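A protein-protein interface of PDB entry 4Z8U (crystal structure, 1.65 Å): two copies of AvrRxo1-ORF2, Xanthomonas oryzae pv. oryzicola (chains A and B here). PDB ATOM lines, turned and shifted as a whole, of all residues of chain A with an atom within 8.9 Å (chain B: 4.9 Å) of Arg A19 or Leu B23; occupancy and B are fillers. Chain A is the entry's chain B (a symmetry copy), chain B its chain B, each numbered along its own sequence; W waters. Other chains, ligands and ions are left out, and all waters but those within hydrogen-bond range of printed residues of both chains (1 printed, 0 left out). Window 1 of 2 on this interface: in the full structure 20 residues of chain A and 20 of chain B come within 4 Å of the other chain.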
ATOM      1  N   PHE A  12     -23.179  36.227  18.351  1.00  0.00           N
ATOM      2  CA  PHE A  12     -24.193  35.873  19.368  1.00  0.00           C
ATOM      3  C   PHE A  12     -25.197  34.856  18.795  1.00  0.00           C
ATOM      4  O   PHE A  12     -25.530  33.842  19.414  1.00  0.00           O
ATOM      5  CB  PHE A  12     -24.913  37.141  19.873  1.00  0.00           C
ATOM      6  CG  PHE A  12     -25.668  36.958  21.186  1.00  0.00           C
ATOM      7  CD1 PHE A  12     -25.035  37.150  22.394  1.00  0.00           C
ATOM      8  CD2 PHE A  12     -26.965  36.509  21.186  1.00  0.00           C
ATOM      9  CE1 PHE A  12     -25.687  36.978  23.610  1.00  0.00           C
ATOM     10  CE2 PHE A  12     -27.656  36.370  22.431  1.00  0.00           C
ATOM     11  CZ  PHE A  12     -27.003  36.652  23.624  1.00  0.00           C
ATOM     12  N   HIS A  13     -25.728  35.137  17.602  1.00  0.00           N
ATOM     13  CA  HIS A  13     -26.731  34.275  16.994  1.00  0.00           C
ATOM     14  C   HIS A  13     -26.151  32.883  16.733  1.00  0.00           C
ATOM     15  O   HIS A  13     -26.739  31.872  17.041  1.00  0.00           O
ATOM     16  CB  HIS A  13     -27.181  34.999  15.688  1.00  0.00           C
ATOM     17  CG  HIS A  13     -28.137  34.203  14.847  1.00  0.00           C
ATOM     18  ND1 HIS A  13     -29.507  34.234  15.065  1.00  0.00           N
ATOM     19  CD2 HIS A  13     -27.935  33.348  13.798  1.00  0.00           C
ATOM     20  CE1 HIS A  13     -30.110  33.492  14.144  1.00  0.00           C
ATOM     21  NE2 HIS A  13     -29.133  32.905  13.361  1.00  0.00           N
ATOM     22  N   LYS A  14     -24.877  32.836  16.267  1.00  0.00           N
ATOM     23  CA  LYS A  14     -24.255  31.534  15.951  1.00  0.00           C
ATOM     24  C   LYS A  14     -24.068  30.679  17.268  1.00  0.00           C
ATOM     25  O   LYS A  14     -24.432  29.483  17.296  1.00  0.00           O
ATOM     26  CB  LYS A  14     -22.789  31.785  15.423  1.00  0.00           C
ATOM     27  CG  LYS A  14     -22.179  30.470  15.000  1.00  0.00           C
ATOM     28  CD  LYS A  14     -20.822  30.838  14.321  1.00  0.00           C
ATOM     29  CE  LYS A  14     -20.209  29.580  13.749  1.00  0.00           C
ATOM     30  NZ  LYS A  14     -18.844  30.008  13.213  1.00  0.00           N
ATOM     31  N   LYS A  15     -23.544  31.302  18.282  1.00  0.00           N
ATOM     32  CA  LYS A  15     -23.369  30.626  19.599  1.00  0.00           C
ATOM     33  C   LYS A  15     -24.715  30.205  20.244  1.00  0.00           C
ATOM     34  O   LYS A  15     -24.845  29.100  20.845  1.00  0.00           O
ATOM     35  CB  LYS A  15     -22.494  31.484  20.543  1.00  0.00           C
ATOM     36  CG  LYS A  15     -21.039  31.613  20.033  1.00  0.00           C
ATOM     37  CD  LYS A  15     -20.380  30.206  19.870  1.00  0.00           C
ATOM     38  CE  LYS A  15     -18.863  30.346  19.612  1.00  0.00           C
ATOM     39  NZ  LYS A  15     -18.360  28.941  19.272  1.00  0.00           N
ATOM     40  N   LEU A  16     -25.724  31.069  20.126  1.00  0.00           N
ATOM     41  CA  LEU A  16     -27.031  30.760  20.656  1.00  0.00           C
ATOM     42  C   LEU A  16     -27.653  29.564  19.919  1.00  0.00           C
ATOM     43  O   LEU A  16     -28.326  28.713  20.502  1.00  0.00           O
ATOM     44  CB  LEU A  16     -27.946  32.016  20.587  1.00  0.00           C
ATOM     45  CG  LEU A  16     -29.340  31.837  21.167  1.00  0.00           C
ATOM     46  CD1 LEU A  16     -29.386  31.367  22.633  1.00  0.00           C
ATOM     47  CD2 LEU A  16     -30.028  33.197  21.021  1.00  0.00           C
ATOM     48  N   LYS A  17     -27.502  29.490  18.581  1.00  0.00           N
ATOM     49  CA  LYS A  17     -27.944  28.352  17.833  1.00  0.00           C
ATOM     50  C   LYS A  17     -27.321  27.045  18.355  1.00  0.00           C
ATOM     51  O   LYS A  17     -28.021  26.043  18.503  1.00  0.00           O
ATOM     52  CB  LYS A  17     -27.608  28.543  16.355  1.00  0.00           C
ATOM     53  CG  LYS A  17     -28.613  29.325  15.541  1.00  0.00           C
ATOM     54  CD  LYS A  17     -28.067  29.573  14.080  1.00  0.00           C
ATOM     55  CE  LYS A  17     -27.949  28.214  13.382  1.00  0.00           C
ATOM     56  NZ  LYS A  17     -27.753  28.522  11.921  1.00  0.00           N
ATOM     57  N   GLU A  18     -26.000  27.094  18.574  1.00  0.00           N
ATOM     58  CA  GLU A  18     -25.321  25.917  19.152  1.00  0.00           C
ATOM     59  C   GLU A  18     -25.856  25.545  20.522  1.00  0.00           C
ATOM     60  O   GLU A  18     -26.026  24.345  20.783  1.00  0.00           O
ATOM     61  CB  GLU A  18     -23.852  26.246  19.317  1.00  0.00           C
ATOM     62  CG  GLU A  18     -23.169  26.480  17.981  1.00  0.00           C
ATOM     63  CD  GLU A  18     -21.656  26.677  18.150  1.00  0.00           C
ATOM     64  OE1 GLU A  18     -21.141  26.549  19.275  1.00  0.00           O
ATOM     65  OE2 GLU A  18     -21.007  27.023  17.137  1.00  0.00           O
ATOM     66  N   ARG A  19     -26.093  26.520  21.399  1.00  0.00           N
ATOM     67  CA  ARG A  19     -26.708  26.269  22.697  1.00  0.00           C
ATOM     68  C   ARG A  19     -28.057  25.627  22.578  1.00  0.00           C
ATOM     69  O   ARG A  19     -28.377  24.609  23.224  1.00  0.00           O
ATOM     70  CB  ARG A  19     -26.806  27.602  23.500  1.00  0.00           C
ATOM     71  CG  ARG A  19     -27.519  27.489  24.874  1.00  0.00           C
ATOM     72  CD  ARG A  19     -27.902  28.854  25.346  1.00  0.00           C
ATOM     73  NE  ARG A  19     -28.372  28.886  26.745  1.00  0.00           N
ATOM     74  CZ  ARG A  19     -27.538  28.945  27.802  1.00  0.00           C
ATOM     75  NH1 ARG A  19     -26.225  29.000  27.684  1.00  0.00           N
ATOM     76  NH2 ARG A  19     -28.014  28.981  29.008  1.00  0.00           N
ATOM     77  N   ASN A  20     -28.927  26.167  21.728  1.00  0.00           N
ATOM     78  CA  ASN A  20     -30.262  25.650  21.666  1.00  0.00           C
ATOM     79  C   ASN A  20     -30.322  24.278  20.938  1.00  0.00           C
ATOM     80  O   ASN A  20     -31.183  23.467  21.208  1.00  0.00           O
ATOM     81  CB  ASN A  20     -31.143  26.669  20.872  1.00  0.00           C
ATOM     82  CG  ASN A  20     -31.452  27.896  21.672  1.00  0.00           C
ATOM     83  OD1 ASN A  20     -31.219  27.948  22.886  1.00  0.00           O
ATOM     84  ND2 ASN A  20     -31.947  28.935  20.975  1.00  0.00           N
ATOM     85  N   LYS A  21     -29.315  24.003  20.085  1.00  0.00           N
ATOM     86  CA  LYS A  21     -29.269  22.718  19.400  1.00  0.00           C
ATOM     87  C   LYS A  21     -28.858  21.619  20.448  1.00  0.00           C
ATOM     88  O   LYS A  21     -29.447  20.514  20.458  1.00  0.00           O
ATOM     89  CB  LYS A  21     -28.083  22.781  18.353  1.00  0.00           C
ATOM     90  CG  LYS A  21     -27.864  21.454  17.597  1.00  0.00           C
ATOM     91  CD  LYS A  21     -26.518  21.505  16.836  1.00  0.00           C
ATOM     92  CE  LYS A  21     -26.476  20.434  15.726  1.00  0.00           C
ATOM     93  NZ  LYS A  21     -25.284  20.589  14.801  1.00  0.00           N
ATOM     94  N   ALA A  22     -27.913  21.986  21.342  1.00  0.00           N
ATOM     95  CA  ALA A  22     -27.561  21.095  22.466  1.00  0.00           C
ATOM     96  C   ALA A  22     -28.726  20.849  23.377  1.00  0.00           C
ATOM     97  O   ALA A  22     -28.983  19.684  23.782  1.00  0.00           O
ATOM     98  CB  ALA A  22     -26.354  21.636  23.276  1.00  0.00           C
ATOM     99  N   LEU A  23     -29.478  21.915  23.710  1.00  0.00           N
ATOM    100  CA  LEU A  23     -30.632  21.774  24.548  1.00  0.00           C
ATOM    101  C   LEU A  23     -31.675  20.888  23.871  1.00  0.00           C
ATOM    102  O   LEU A  23     -32.369  20.068  24.544  1.00  0.00           O
ATOM    103  CB  LEU A  23     -31.232  23.118  24.963  1.00  0.00           C
ATOM    104  CG  LEU A  23     -30.420  23.966  25.958  1.00  0.00           C
ATOM    105  CD1 LEU A  23     -30.943  25.404  26.034  1.00  0.00           C
ATOM    106  CD2 LEU A  23     -30.694  23.343  27.339  1.00  0.00           C
ATOM    107  N   HIS A  24     -31.849  21.091  22.547  1.00  0.00           N
ATOM    108  CA  HIS A  24     -32.886  20.345  21.771  1.00  0.00           C
ATOM    109  C   HIS A  24     -32.556  18.855  21.847  1.00  0.00           C
ATOM    110  O   HIS A  24     -33.436  18.032  22.147  1.00  0.00           O
ATOM    111  CB  HIS A  24     -32.826  20.867  20.326  1.00  0.00           C
ATOM    112  CG  HIS A  24     -33.939  20.389  19.404  1.00  0.00           C
ATOM    113  ND1 HIS A  24     -35.245  20.836  19.530  1.00  0.00           N
ATOM    114  CD2 HIS A  24     -33.910  19.517  18.341  1.00  0.00           C
ATOM    115  CE1 HIS A  24     -35.995  20.248  18.572  1.00  0.00           C
ATOM    116  NE2 HIS A  24     -35.165  19.447  17.828  1.00  0.00           N
ATOM    117  N   ALA A  25     -31.320  18.510  21.511  1.00  0.00           N
ATOM    118  CA  ALA A  25     -30.898  17.124  21.534  1.00  0.00           C
ATOM    119  C   ALA A  25     -31.031  16.549  22.983  1.00  0.00           C
ATOM    120  O   ALA A  25     -31.566  15.468  23.152  1.00  0.00           O
ATOM    121  CB  ALA A  25     -29.464  17.065  21.096  1.00  0.00           C
ATOM    122  N   SER A  26     -30.581  17.331  23.971  1.00  0.00           N
ATOM    123  CA  SER A  26     -30.594  16.859  25.357  1.00  0.00           C
ATOM    124  C   SER A  26     -31.999  16.562  25.867  1.00  0.00           C
ATOM    125  O   SER A  26     -32.259  15.543  26.527  1.00  0.00           O
ATOM    126  CB  SER A  26     -29.886  17.921  26.267  1.00  0.00           C
ATOM    127  OG  SER A  26     -30.037  17.474  27.543  1.00  0.00           O
ATOM    128  N   ASP A  27     -32.945  17.488  25.613  1.00  0.00           N
ATOM    129  CA  ASP A  27     -34.297  17.278  26.068  1.00  0.00           C
ATOM    130  C   ASP A  27     -34.816  15.896  25.621  1.00  0.00           C
ATOM    131  O   ASP A  27     -35.554  15.228  26.361  1.00  0.00           O
ATOM    132  CB  ASP A  27     -35.231  18.348  25.460  1.00  0.00           C
ATOM    133  CG  ASP A  27     -35.114  19.703  26.138  1.00  0.00           C
ATOM    134  OD1 ASP A  27     -34.538  19.814  27.251  1.00  0.00           O
ATOM    135  OD2 ASP A  27     -35.540  20.706  25.452  1.00  0.00           O
ATOM    136  N   LEU A  30     -32.773  12.902  27.470  1.00  0.00           N
ATOM    137  CA  LEU A  30     -33.227  12.675  28.802  1.00  0.00           C
ATOM    138  C   LEU A  30     -34.661  12.161  28.895  1.00  0.00           C
ATOM    139  O   LEU A  30     -34.956  11.320  29.745  1.00  0.00           O
ATOM    140  CB  LEU A  30     -33.129  14.034  29.603  1.00  0.00           C
ATOM    141  CG  LEU A  30     -31.702  14.565  29.697  1.00  0.00           C
ATOM    142  CD1 LEU A  30     -31.833  15.895  30.391  1.00  0.00           C
ATOM    143  CD2 LEU A  30     -30.863  13.582  30.572  1.00  0.00           C
ATOM    144  N   ARG B  19     -25.365  17.786  28.728  1.00  0.00           N
ATOM    145  CA  ARG B  19     -26.190  18.988  28.706  1.00  0.00           C
ATOM    146  C   ARG B  19     -25.580  20.118  29.480  1.00  0.00           C
ATOM    147  O   ARG B  19     -25.458  21.266  29.009  1.00  0.00           O
ATOM    148  CB  ARG B  19     -27.614  18.660  29.251  1.00  0.00           C
ATOM    149  CG  ARG B  19     -28.572  19.875  29.358  1.00  0.00           C
ATOM    150  CD  ARG B  19     -29.723  19.523  30.244  1.00  0.00           C
ATOM    151  NE  ARG B  19     -30.811  20.521  30.226  1.00  0.00           N
ATOM    152  CZ  ARG B  19     -31.772  20.546  29.282  1.00  0.00           C
ATOM    153  NH1 ARG B  19     -31.842  19.669  28.298  1.00  0.00           N
ATOM    154  NH2 ARG B  19     -32.709  21.442  29.327  1.00  0.00           N
ATOM    155  N   ASN B  20     -25.136  19.859  30.707  1.00  0.00           N
ATOM    156  CA  ASN B  20     -24.647  20.934  31.518  1.00  0.00           C
ATOM    157  C   ASN B  20     -23.243  21.420  31.056  1.00  0.00           C
ATOM    158  O   ASN B  20     -22.891  22.568  31.237  1.00  0.00           O
ATOM    159  CB  ASN B  20     -24.532  20.421  32.991  1.00  0.00           C
ATOM    160  CG  ASN B  20     -25.868  20.280  33.649  1.00  0.00           C
ATOM    161  OD1 ASN B  20     -26.890  20.750  33.134  1.00  0.00           O
ATOM    162  ND2 ASN B  20     -25.881  19.577  34.795  1.00  0.00           N
ATOM    163  N   LYS B  21     -22.500  20.539  30.358  1.00  0.00           N
ATOM    164  CA  LYS B  21     -21.195  20.931  29.845  1.00  0.00           C
ATOM    165  C   LYS B  21     -21.418  21.907  28.631  1.00  0.00           C
ATOM    166  O   LYS B  21     -20.710  22.933  28.516  1.00  0.00           O
ATOM    167  CB  LYS B  21     -20.514  19.636  29.239  1.00  0.00           C
ATOM    168  CG  LYS B  21     -19.144  19.914  28.587  1.00  0.00           C
ATOM    169  CD  LYS B  21     -18.700  18.682  27.763  1.00  0.00           C
ATOM    170  CE  LYS B  21     -17.182  18.723  27.490  1.00  0.00           C
ATOM    171  NZ  LYS B  21     -16.655  17.433  26.892  1.00  0.00           N
ATOM    172  N   ALA B  22     -22.443  21.593  27.808  1.00  0.00           N
ATOM    173  CA  ALA B  22     -22.845  22.517  26.729  1.00  0.00           C
ATOM    174  C   ALA B  22     -23.311  23.839  27.262  1.00  0.00           C
ATOM    175  O   ALA B  22     -22.915  24.913  26.735  1.00  0.00           O
ATOM    176  CB  ALA B  22     -23.932  21.897  25.813  1.00  0.00           C
ATOM    177  N   LEU B  23     -24.134  23.814  28.326  1.00  0.00           N
ATOM    178  CA  LEU B  23     -24.605  25.027  28.927  1.00  0.00           C
ATOM    179  C   LEU B  23     -23.434  25.828  29.490  1.00  0.00           C
ATOM    180  O   LEU B  23     -23.415  27.094  29.415  1.00  0.00           O
ATOM    181  CB  LEU B  23     -25.675  24.787  29.992  1.00  0.00           C
ATOM    182  CG  LEU B  23     -27.055  24.312  29.499  1.00  0.00           C
ATOM    183  CD1 LEU B  23     -27.917  23.790  30.652  1.00  0.00           C
ATOM    184  CD2 LEU B  23     -27.759  25.581  28.985  1.00  0.00           C
ATOM    185  N   HIS B  24     -22.481  25.112  30.125  1.00  0.00           N
ATOM    186  CA  HIS B  24     -21.315  25.772  30.786  1.00  0.00           C
ATOM    187  C   HIS B  24     -20.523  26.521  29.715  1.00  0.00           C
ATOM    188  O   HIS B  24     -20.186  27.703  29.896  1.00  0.00           O
ATOM    189  CB  HIS B  24     -20.479  24.658  31.437  1.00  0.00           C
ATOM    190  CG  HIS B  24     -19.348  25.125  32.343  1.00  0.00           C
ATOM    191  ND1 HIS B  24     -19.584  25.696  33.584  1.00  0.00           N
ATOM    192  CD2 HIS B  24     -17.984  25.078  32.172  1.00  0.00           C
ATOM    193  CE1 HIS B  24     -18.396  25.995  34.153  1.00  0.00           C
ATOM    194  NE2 HIS B  24     -17.409  25.595  33.287  1.00  0.00           N
ATOM    195  N   ALA B  25     -20.173  25.819  28.647  1.00  0.00           N
ATOM    196  CA  ALA B  25     -19.408  26.422  27.573  1.00  0.00           C
ATOM    197  C   ALA B  25     -20.209  27.614  26.952  1.00  0.00           C
ATOM    198  O   ALA B  25     -19.649  28.678  26.759  1.00  0.00           O
ATOM    199  CB  ALA B  25     -19.167  25.375  26.525  1.00  0.00           C
ATOM    200  N   SER B  26     -21.508  27.391  26.715  1.00  0.00           N
ATOM    201  CA  SER B  26     -22.332  28.417  26.070  1.00  0.00           C
ATOM    202  C   SER B  26     -22.422  29.701  26.886  1.00  0.00           C
ATOM    203  O   SER B  26     -22.318  30.822  26.363  1.00  0.00           O
ATOM    204  CB  SER B  26     -23.760  27.830  25.798  1.00  0.00           C
ATOM    205  OG  SER B  26     -24.497  28.863  25.309  1.00  0.00           O
ATOM    206  N   ASP B  27     -22.676  29.567  28.203  1.00  0.00           N
ATOM    207  CA  ASP B  27     -22.781  30.738  29.037  1.00  0.00           C
ATOM    208  C   ASP B  27     -21.550  31.650  28.855  1.00  0.00           C
ATOM    209  O   ASP B  27     -21.670  32.885  28.874  1.00  0.00           O
ATOM    210  CB  ASP B  27     -22.838  30.323  30.524  1.00  0.00           C
ATOM    211  CG  ASP B  27     -24.197  29.788  30.946  1.00  0.00           C
ATOM    212  OD1 ASP B  27     -25.207  29.965  30.218  1.00  0.00           O
ATOM    213  OD2 ASP B  27     -24.204  29.070  32.016  1.00  0.00           O
ATOM    214  N   LEU B  30     -21.449  33.228  25.105  1.00  0.00           N
ATOM    215  CA  LEU B  30     -22.331  34.339  24.958  1.00  0.00           C
ATOM    216  C   LEU B  30     -21.957  35.552  25.804  1.00  0.00           C
ATOM    217  O   LEU B  30     -22.106  36.687  25.347  1.00  0.00           O
ATOM    218  CB  LEU B  30     -23.787  33.877  25.360  1.00  0.00           C
ATOM    219  CG  LEU B  30     -24.321  32.754  24.474  1.00  0.00           C
ATOM    220  CD1 LEU B  30     -25.652  32.391  25.076  1.00  0.00           C
ATOM    221  CD2 LEU B  30     -24.518  33.314  23.030  1.00  0.00           C
HETATM  222  O   HOH W   1     -23.208  29.116  22.975  1.00  0.00           O
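Of the printed residues of chain B, Lys A15 touches Leu B30 (3.7 Å). Printed residues of chain B within 4 Å of Arg A19: Leu B23 (3.4 Å), Ser B26 (2.9 Å) and Asp B27 (2.9 Å). Printed residues of chain B within 4 Å of Leu A23: Arg B19 (3.4 Å). Ala A25 touches none of the printed residues of chain B. Of the printed residues of chain B, Ser A26 touches Arg B19 (2.9 Å). Ala B22 touches just one residue of chain A: Ala A22 (3.5 Å). Of chain A, only Arg A19 (3.4 Å) comes within 4 Å of Leu B23. The nearest residue of chain B that does not touch Arg A19 is Leu B30 (4.2 Å). The nearest printed residue of chain B that does not touch Ser A26 is Asn B20 (6.3 Å).
Of the 17 printed residues of chain A, 8 touch a printed residue of chain B. Hydrophobic or aromatic side chains of chain B that line the printed part of chain A: Ala B22, Leu B23 and Leu B30. Among the printed residues, 10 pairs touch across the chains. Among the printed residues, Asp or Glu carboxylates within 4 Å of a Lys or Arg side-chain nitrogen of the other chain: Arg A19 with Asp B27 (2.9 Å) and Asp A27 with Arg B19 (2.9 Å).
Arg A19 touches Leu B23, and with the chains exchanged Leu A23 touches Arg B19. Arg A19 touches Ser B26, and with the chains exchanged Ser A26 touches Arg B19. Arg A19 touches Asp B27, and with the chains exchanged Asp A27 touches Arg B19. Ala A22 touches its own counterpart, Ala B22. Positions printed for both chains: 19, 20, 21, 22, 23, 24, 25, 26, 27 and 30. Of the 10 pairs that touch across the chains among the printed residues, 7 have their exchanged pair printed and touching as well.
Water W1 bridges OG of Ser B26 (2.7 Å) and O of Lys A15 (2.7 Å).
NZ of Lys A15 is in salt-bridge range of OE1 of Glu A18 (3.7 Å).
Among the printed residues, merely in contact across the chains: Arg A19 with Leu B23, Leu A23 with Arg B19, Ala A22 with Ala B22, Lys A15 with Leu B30, Phe A12 with Leu B30 and Leu A16 with Leu B30.
The side-chain hydroxyl of Ser A26 sits at hydrogen-bond distance from the guanidinium group of Arg B19 (2.9 Å). NH1 of Arg B19 is in salt-bridge range of OD1 of Asp A27 (2.9 Å). OG of Ser B26 is in hydrogen-bond range of NH1 of Arg A19 (2.9 Å). NH1 of Arg A19 is in salt-bridge range of OD1 of Asp B27 (2.9 Å).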
